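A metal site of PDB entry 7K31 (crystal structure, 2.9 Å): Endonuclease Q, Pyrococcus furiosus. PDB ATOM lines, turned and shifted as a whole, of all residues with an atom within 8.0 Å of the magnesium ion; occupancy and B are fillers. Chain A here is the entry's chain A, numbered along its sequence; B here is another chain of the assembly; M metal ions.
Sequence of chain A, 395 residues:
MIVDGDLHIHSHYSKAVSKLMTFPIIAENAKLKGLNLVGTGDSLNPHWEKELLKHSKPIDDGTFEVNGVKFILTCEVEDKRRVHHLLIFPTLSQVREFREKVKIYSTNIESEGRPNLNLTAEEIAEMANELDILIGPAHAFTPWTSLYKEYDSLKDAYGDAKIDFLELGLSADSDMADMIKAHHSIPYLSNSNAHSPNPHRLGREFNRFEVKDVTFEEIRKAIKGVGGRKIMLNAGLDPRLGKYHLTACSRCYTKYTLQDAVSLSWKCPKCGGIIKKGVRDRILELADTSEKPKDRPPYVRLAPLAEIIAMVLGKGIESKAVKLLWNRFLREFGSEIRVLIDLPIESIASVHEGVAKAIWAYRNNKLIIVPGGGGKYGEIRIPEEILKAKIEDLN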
ATOM      1  N   LEU A 168      -0.898  20.972  12.841  1.00  0.00           N
ATOM      2  CA  LEU A 168      -1.818  22.097  12.644  1.00  0.00           C
ATOM      3  C   LEU A 168      -1.631  23.152  13.714  1.00  0.00           C
ATOM      4  O   LEU A 168      -1.532  24.346  13.409  1.00  0.00           O
ATOM      5  CB  LEU A 168      -3.255  21.599  12.640  1.00  0.00           C
ATOM      6  CG  LEU A 168      -3.694  20.785  11.421  1.00  0.00           C
ATOM      7  CD1 LEU A 168      -5.165  20.446  11.519  1.00  0.00           C
ATOM      8  CD2 LEU A 168      -3.405  21.570  10.160  1.00  0.00           C
ATOM      9  N   GLY A 169      -1.600  22.750  14.968  1.00  0.00           N
ATOM     10  CA  GLY A 169      -1.512  23.673  16.078  1.00  0.00           C
ATOM     11  C   GLY A 169      -2.867  23.919  16.732  1.00  0.00           C
ATOM     12  O   GLY A 169      -3.935  23.561  16.213  1.00  0.00           O
ATOM     13  N   LEU A 170      -2.805  24.540  17.909  1.00  0.00           N
ATOM     14  CA  LEU A 170      -4.022  24.822  18.668  1.00  0.00           C
ATOM     15  C   LEU A 170      -4.968  25.696  17.868  1.00  0.00           C
ATOM     16  O   LEU A 170      -6.119  25.317  17.591  1.00  0.00           O
ATOM     17  CB  LEU A 170      -3.653  25.471  20.002  1.00  0.00           C
ATOM     18  CG  LEU A 170      -3.289  24.579  21.191  1.00  0.00           C
ATOM     19  CD1 LEU A 170      -2.205  23.584  20.856  1.00  0.00           C
ATOM     20  CD2 LEU A 170      -2.860  25.439  22.370  1.00  0.00           C
ATOM     21  N   SER A 171      -4.499  26.875  17.454  1.00  0.00           N
ATOM     22  CA  SER A 171      -5.284  27.924  16.817  1.00  0.00           C
ATOM     23  C   SER A 171      -5.694  27.620  15.386  1.00  0.00           C
ATOM     24  O   SER A 171      -6.208  28.537  14.728  1.00  0.00           O
ATOM     25  CB  SER A 171      -4.526  29.247  16.866  1.00  0.00           C
ATOM     26  OG  SER A 171      -4.190  29.592  18.192  1.00  0.00           O
ATOM     27  N   ALA A 172      -5.500  26.411  14.858  1.00  0.00           N
ATOM     28  CA  ALA A 172      -5.914  26.088  13.503  1.00  0.00           C
ATOM     29  C   ALA A 172      -6.675  24.775  13.494  1.00  0.00           C
ATOM     30  O   ALA A 172      -6.541  23.943  14.398  1.00  0.00           O
ATOM     31  CB  ALA A 172      -4.720  26.017  12.547  1.00  0.00           C
ATOM     32  N   ASP A 173      -7.503  24.598  12.462  1.00  0.00           N
ATOM     33  CA  ASP A 173      -8.157  23.327  12.176  1.00  0.00           C
ATOM     34  C   ASP A 173      -7.868  22.952  10.717  1.00  0.00           C
ATOM     35  O   ASP A 173      -7.196  23.688   9.986  1.00  0.00           O
ATOM     36  CB  ASP A 173      -9.656  23.365  12.514  1.00  0.00           C
ATOM     37  CG  ASP A 173     -10.469  24.152  11.510  1.00  0.00           C
ATOM     38  OD1 ASP A 173      -9.915  25.048  10.840  1.00  0.00           O
ATOM     39  OD2 ASP A 173     -11.687  23.886  11.393  1.00  0.00           O
ATOM     40  N   SER A 174      -8.384  21.802  10.291  1.00  0.00           N
ATOM     41  CA  SER A 174      -7.996  21.255   8.999  1.00  0.00           C
ATOM     42  C   SER A 174      -8.491  22.117   7.844  1.00  0.00           C
ATOM     43  O   SER A 174      -7.816  22.172   6.798  1.00  0.00           O
ATOM     44  CB  SER A 174      -8.481  19.815   8.845  1.00  0.00           C
ATOM     45  OG  SER A 174      -7.917  18.972   9.837  1.00  0.00           O
ATOM     46  N   MET A 176      -9.081  25.606   7.620  1.00  0.00           N
ATOM     47  CA  MET A 176      -8.313  26.831   7.401  1.00  0.00           C
ATOM     48  C   MET A 176      -6.886  26.521   6.959  1.00  0.00           C
ATOM     49  O   MET A 176      -6.304  27.293   6.195  1.00  0.00           O
ATOM     50  CB  MET A 176      -8.361  27.736   8.639  1.00  0.00           C
ATOM     51  CG  MET A 176      -7.803  27.126   9.907  1.00  0.00           C
ATOM     52  SD  MET A 176      -8.088  28.198  11.321  1.00  0.00           S
ATOM     53  CE  MET A 176      -9.878  28.237  11.377  1.00  0.00           C
ATOM     54  N   LEU A 189      -1.407  16.540  11.404  1.00  0.00           N
ATOM     55  CA  LEU A 189      -1.312  16.078  12.773  1.00  0.00           C
ATOM     56  C   LEU A 189      -1.830  17.170  13.689  1.00  0.00           C
ATOM     57  O   LEU A 189      -1.523  18.350  13.488  1.00  0.00           O
ATOM     58  CB  LEU A 189       0.124  15.732  13.158  1.00  0.00           C
ATOM     59  CG  LEU A 189       0.717  14.485  12.494  1.00  0.00           C
ATOM     60  CD1 LEU A 189       2.055  14.162  13.127  1.00  0.00           C
ATOM     61  CD2 LEU A 189      -0.244  13.316  12.621  1.00  0.00           C
ATOM     62  N   SER A 190      -2.612  16.780  14.686  1.00  0.00           N
ATOM     63  CA  SER A 190      -3.119  17.688  15.701  1.00  0.00           C
ATOM     64  C   SER A 190      -2.629  17.150  17.038  1.00  0.00           C
ATOM     65  O   SER A 190      -3.196  16.208  17.586  1.00  0.00           O
ATOM     66  CB  SER A 190      -4.638  17.767  15.652  1.00  0.00           C
ATOM     67  OG  SER A 190      -5.217  16.472  15.616  1.00  0.00           O
ATOM     68  N   ASN A 191      -1.563  17.743  17.556  1.00  0.00           N
ATOM     69  CA  ASN A 191      -0.940  17.310  18.804  1.00  0.00           C
ATOM     70  C   ASN A 191      -1.117  18.380  19.883  1.00  0.00           C
ATOM     71  O   ASN A 191      -1.653  19.465  19.629  1.00  0.00           O
ATOM     72  CB  ASN A 191       0.530  16.975  18.564  1.00  0.00           C
ATOM     73  CG  ASN A 191       0.721  15.870  17.552  1.00  0.00           C
ATOM     74  OD1 ASN A 191      -0.002  14.873  17.578  1.00  0.00           O
ATOM     75  ND2 ASN A 191       1.682  16.042  16.663  1.00  0.00           N
ATOM     76  N   ARG A 204      -4.613  17.539  24.801  1.00  0.00           N
ATOM     77  CA  ARG A 204      -5.633  18.508  24.434  1.00  0.00           C
ATOM     78  C   ARG A 204      -6.016  18.373  22.971  1.00  0.00           C
ATOM     79  O   ARG A 204      -7.167  18.657  22.587  1.00  0.00           O
ATOM     80  CB  ARG A 204      -5.159  19.931  24.740  1.00  0.00           C
ATOM     81  CG  ARG A 204      -3.875  20.323  24.044  1.00  0.00           C
ATOM     82  CD  ARG A 204      -3.869  21.792  23.681  1.00  0.00           C
ATOM     83  NE  ARG A 204      -3.449  22.638  24.791  1.00  0.00           N
ATOM     84  CZ  ARG A 204      -2.203  23.065  24.978  1.00  0.00           C
ATOM     85  NH1 ARG A 204      -1.251  22.715  24.125  1.00  0.00           N
ATOM     86  NH2 ARG A 204      -1.919  23.833  26.011  1.00  0.00           N
ATOM     87  N   GLU A 205      -5.068  17.957  22.126  1.00  0.00           N
ATOM     88  CA  GLU A 205      -5.320  17.545  20.748  1.00  0.00           C
ATOM     89  C   GLU A 205      -4.725  16.154  20.562  1.00  0.00           C
ATOM     90  O   GLU A 205      -3.773  15.776  21.249  1.00  0.00           O
ATOM     91  CB  GLU A 205      -4.681  18.512  19.738  1.00  0.00           C
ATOM     92  CG  GLU A 205      -5.014  19.995  19.930  1.00  0.00           C
ATOM     93  CD  GLU A 205      -4.868  20.802  18.639  1.00  0.00           C
ATOM     94  OE1 GLU A 205      -4.035  20.435  17.780  1.00  0.00           O
ATOM     95  OE2 GLU A 205      -5.597  21.812  18.471  1.00  0.00           O
ATOM     96  N   ASN A 234      -9.080  13.645  13.450  1.00  0.00           N
ATOM     97  CA  ASN A 234      -8.163  14.674  13.939  1.00  0.00           C
ATOM     98  C   ASN A 234      -8.908  15.465  15.020  1.00  0.00           C
ATOM     99  O   ASN A 234      -9.703  16.347  14.686  1.00  0.00           O
ATOM    100  CB  ASN A 234      -7.746  15.596  12.797  1.00  0.00           C
ATOM    101  CG  ASN A 234      -6.324  15.344  12.342  1.00  0.00           C
ATOM    102  OD1 ASN A 234      -6.059  15.148  11.151  1.00  0.00           O
ATOM    103  ND2 ASN A 234      -5.384  15.385  13.281  1.00  0.00           N
ATOM    104  N   ALA A 235      -8.669  15.168  16.295  1.00  0.00           N
ATOM    105  CA  ALA A 235      -9.319  15.888  17.369  1.00  0.00           C
ATOM    106  C   ALA A 235      -8.389  16.976  17.886  1.00  0.00           C
ATOM    107  O   ALA A 235      -7.175  16.777  17.993  1.00  0.00           O
ATOM    108  CB  ALA A 235      -9.696  14.946  18.513  1.00  0.00           C
ATOM    109  N   GLY A 236      -8.947  18.135  18.209  1.00  0.00           N
ATOM    110  CA  GLY A 236      -8.103  19.247  18.598  1.00  0.00           C
ATOM    111  C   GLY A 236      -8.887  20.353  19.255  1.00  0.00           C
ATOM    112  O   GLY A 236     -10.118  20.355  19.279  1.00  0.00           O
ATOM    113  N   LEU A 237      -8.136  21.308  19.803  1.00  0.00           N
ATOM    114  CA  LEU A 237      -8.732  22.492  20.396  1.00  0.00           C
ATOM    115  C   LEU A 237      -9.391  23.337  19.308  1.00  0.00           C
ATOM    116  O   LEU A 237      -8.848  23.482  18.213  1.00  0.00           O
ATOM    117  CB  LEU A 237      -7.653  23.317  21.089  1.00  0.00           C
ATOM    118  CG  LEU A 237      -7.830  23.529  22.588  1.00  0.00           C
ATOM    119  CD1 LEU A 237      -7.764  22.200  23.319  1.00  0.00           C
ATOM    120  CD2 LEU A 237      -6.782  24.493  23.127  1.00  0.00           C
ATOM    121  N   ASP A 238     -10.558  23.871  19.634  1.00  0.00           N
ATOM    122  CA  ASP A 238     -11.231  24.816  18.748  1.00  0.00           C
ATOM    123  C   ASP A 238     -10.263  25.939  18.397  1.00  0.00           C
ATOM    124  O   ASP A 238      -9.605  26.480  19.302  1.00  0.00           O
ATOM    125  CB  ASP A 238     -12.458  25.392  19.461  1.00  0.00           C
ATOM    126  CG  ASP A 238     -13.310  26.272  18.566  1.00  0.00           C
ATOM    127  OD1 ASP A 238     -12.804  27.299  18.068  1.00  0.00           O
ATOM    128  OD2 ASP A 238     -14.491  25.940  18.350  1.00  0.00           O
ATOM    129  N   PRO A 239     -10.123  26.301  17.122  1.00  0.00           N
ATOM    130  CA  PRO A 239      -9.103  27.283  16.735  1.00  0.00           C
ATOM    131  C   PRO A 239      -9.171  28.585  17.510  1.00  0.00           C
ATOM    132  O   PRO A 239      -8.131  29.217  17.742  1.00  0.00           O
ATOM    133  CB  PRO A 239      -9.376  27.500  15.236  1.00  0.00           C
ATOM    134  CG  PRO A 239     -10.048  26.245  14.792  1.00  0.00           C
ATOM    135  CD  PRO A 239     -10.872  25.781  15.959  1.00  0.00           C
ATOM    136  N   ARG A 240     -10.364  29.000  17.946  1.00  0.00           N
ATOM    137  CA  ARG A 240     -10.495  30.279  18.632  1.00  0.00           C
ATOM    138  C   ARG A 240      -9.901  30.260  20.026  1.00  0.00           C
ATOM    139  O   ARG A 240      -9.551  31.321  20.550  1.00  0.00           O
ATOM    140  CB  ARG A 240     -11.967  30.696  18.672  1.00  0.00           C
ATOM    141  CG  ARG A 240     -12.591  30.867  17.294  1.00  0.00           C
ATOM    142  CD  ARG A 240     -14.042  31.301  17.379  1.00  0.00           C
ATOM    143  NE  ARG A 240     -14.907  30.241  17.884  1.00  0.00           N
ATOM    144  CZ  ARG A 240     -15.528  29.352  17.121  1.00  0.00           C
ATOM    145  NH1 ARG A 240     -15.371  29.385  15.796  1.00  0.00           N
ATOM    146  NH2 ARG A 240     -16.300  28.429  17.663  1.00  0.00           N
ATOM    147  N   LEU A 241      -9.745  29.086  20.644  1.00  0.00           N
ATOM    148  CA  LEU A 241      -9.208  29.008  21.996  1.00  0.00           C
ATOM    149  C   LEU A 241      -7.697  29.172  22.043  1.00  0.00           C
ATOM    150  O   LEU A 241      -7.145  29.305  23.138  1.00  0.00           O
ATOM    151  CB  LEU A 241      -9.603  27.683  22.647  1.00  0.00           C
ATOM    152  CG  LEU A 241     -11.091  27.363  22.762  1.00  0.00           C
ATOM    153  CD1 LEU A 241     -11.302  26.078  23.542  1.00  0.00           C
ATOM    154  CD2 LEU A 241     -11.839  28.510  23.418  1.00  0.00           C
ATOM    155  N   GLY A 242      -7.013  29.166  20.900  1.00  0.00           N
ATOM    156  CA  GLY A 242      -5.568  29.143  20.894  1.00  0.00           C
ATOM    157  C   GLY A 242      -4.945  30.441  21.350  1.00  0.00           C
ATOM    158  O   GLY A 242      -5.561  31.504  21.371  1.00  0.00           O
ATOM    159  N   TYR A 299     -12.179  16.998  11.351  1.00  0.00           N
ATOM    160  CA  TYR A 299     -11.550  17.665  12.492  1.00  0.00           C
ATOM    161  C   TYR A 299     -12.653  17.979  13.495  1.00  0.00           C
ATOM    162  O   TYR A 299     -13.513  18.830  13.229  1.00  0.00           O
ATOM    163  CB  TYR A 299     -10.830  18.932  12.055  1.00  0.00           C
ATOM    164  CG  TYR A 299      -9.928  19.552  13.106  1.00  0.00           C
ATOM    165  CD1 TYR A 299     -10.463  20.346  14.119  1.00  0.00           C
ATOM    166  CD2 TYR A 299      -8.551  19.366  13.081  1.00  0.00           C
ATOM    167  CE1 TYR A 299      -9.649  20.922  15.081  1.00  0.00           C
ATOM    168  CE2 TYR A 299      -7.737  19.943  14.044  1.00  0.00           C
ATOM    169  CZ  TYR A 299      -8.282  20.723  15.042  1.00  0.00           C
ATOM    170  OH  TYR A 299      -7.476  21.304  15.993  1.00  0.00           O
ATOM    171  N   VAL A 300     -12.640  17.291  14.632  1.00  0.00           N
ATOM    172  CA  VAL A 300     -13.611  17.515  15.684  1.00  0.00           C
ATOM    173  C   VAL A 300     -13.019  18.552  16.629  1.00  0.00           C
ATOM    174  O   VAL A 300     -12.061  18.281  17.347  1.00  0.00           O
ATOM    175  CB  VAL A 300     -13.957  16.216  16.426  1.00  0.00           C
ATOM    176  CG1 VAL A 300     -15.242  15.624  15.876  1.00  0.00           C
ATOM    177  CG2 VAL A 300     -12.827  15.230  16.265  1.00  0.00           C
ATOM    178  N   ARG A 301     -13.592  19.758  16.616  1.00  0.00           N
ATOM    179  CA  ARG A 301     -13.175  20.797  17.545  1.00  0.00           C
ATOM    180  C   ARG A 301     -13.696  20.469  18.935  1.00  0.00           C
ATOM    181  O   ARG A 301     -14.873  20.133  19.094  1.00  0.00           O
ATOM    182  CB  ARG A 301     -13.730  22.152  17.103  1.00  0.00           C
ATOM    183  CG  ARG A 301     -13.338  22.572  15.706  1.00  0.00           C
ATOM    184  CD  ARG A 301     -14.001  23.890  15.341  1.00  0.00           C
ATOM    185  NE  ARG A 301     -13.512  24.427  14.076  1.00  0.00           N
ATOM    186  CZ  ARG A 301     -13.884  25.588  13.554  1.00  0.00           C
ATOM    187  NH1 ARG A 301     -14.776  26.341  14.192  1.00  0.00           N
ATOM    188  NH2 ARG A 301     -13.372  25.995  12.407  1.00  0.00           N
ATOM    189  N   LEU A 302     -12.833  20.572  19.937  1.00  0.00           N
ATOM    190  CA  LEU A 302     -13.236  20.304  21.304  1.00  0.00           C
ATOM    191  C   LEU A 302     -12.625  21.340  22.236  1.00  0.00           C
ATOM    192  O   LEU A 302     -11.518  21.844  21.995  1.00  0.00           O
ATOM    193  CB  LEU A 302     -12.881  18.872  21.757  1.00  0.00           C
ATOM    194  CG  LEU A 302     -11.440  18.397  21.648  1.00  0.00           C
ATOM    195  CD1 LEU A 302     -10.607  18.792  22.871  1.00  0.00           C
ATOM    196  CD2 LEU A 302     -11.415  16.891  21.450  1.00  0.00           C
ATOM    197  P    DI B  14       6.802  24.931  22.615  1.00  0.00           P
ATOM    198  OP1  DI B  14       6.987  23.478  22.567  1.00  0.00           O
ATOM    199  OP2  DI B  14       7.121  25.242  21.266  1.00  0.00           O
ATOM    200  O5'  DI B  14       5.540  25.614  22.948  1.00  0.00           O
ATOM    201  C5'  DI B  14       4.558  25.786  22.002  1.00  0.00           C
ATOM    202  C4'  DI B  14       3.572  26.733  22.572  1.00  0.00           C
ATOM    203  O4'  DI B  14       2.762  27.130  21.569  1.00  0.00           O
ATOM    204  C3'  DI B  14       2.698  25.853  23.266  1.00  0.00           C
ATOM    205  O3'  DI B  14       1.906  26.561  24.148  1.00  0.00           O
ATOM    206  C2'  DI B  14       1.858  25.312  22.183  1.00  0.00           C
ATOM    207  C1'  DI B  14       1.499  26.575  21.615  1.00  0.00           C
ATOM    208  N9   DI B  14       0.851  26.311  20.426  1.00  0.00           N
ATOM    209  C8   DI B  14       0.902  25.279  19.726  1.00  0.00           C
ATOM    210  N7   DI B  14       0.108  25.480  18.726  1.00  0.00           N
ATOM    211  C5   DI B  14      -0.454  26.603  18.845  1.00  0.00           C
ATOM    212  C6   DI B  14      -1.358  27.410  18.154  1.00  0.00           C
ATOM    213  O6   DI B  14      -1.793  27.011  17.130  1.00  0.00           O
ATOM    214  N1   DI B  14      -1.722  28.544  18.620  1.00  0.00           N
ATOM    215  C2   DI B  14      -1.192  28.959  19.709  1.00  0.00           C
ATOM    216  N3   DI B  14      -0.341  28.294  20.403  1.00  0.00           N
ATOM    217  C4   DI B  14       0.038  27.138  19.998  1.00  0.00           C
HETATM  218 MG    MG M   1      -6.455  22.956  16.804  1.00  0.00          MG
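The side-chain hydroxyl of Tyr 299 lies close to the backbone carbonyl oxygen of Ala 172, 3.2 Å away.
OH of Tyr 299 lies close to O of Leu 237 (3.4 Å).
The side-chain carboxylate of Glu 205 sits close to the backbone NH of Leu 237 (2.9 Å).
N of Leu 170 is in hydrogen-bond range of O6 of DI 14 of chain B (2.8 Å).
Along chain A the residues within 4 Å of the magnesium ion span positions 169 to 299.
The nearest printed residue that does not touch the magnesium ion is Gly 236 (4.3 Å).
The magnesium ion is bound by OH of Tyr 299 (2.1 Å), OE2 of Glu 205 (2.2 Å) and O of Leu 170 (2.5 Å).
The magnesium ion has three donor atoms within binding distance.
Slightly farther from the magnesium ion lies the backbone carbonyl oxygen (O) of Ala 172 (2.6 Å).
Slightly farther from the magnesium ion lies O of Gly 169 (2.7 Å).
Slightly farther from the magnesium ion lies the backbone carbonyl oxygen (O) of Leu 237 (2.8 Å).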
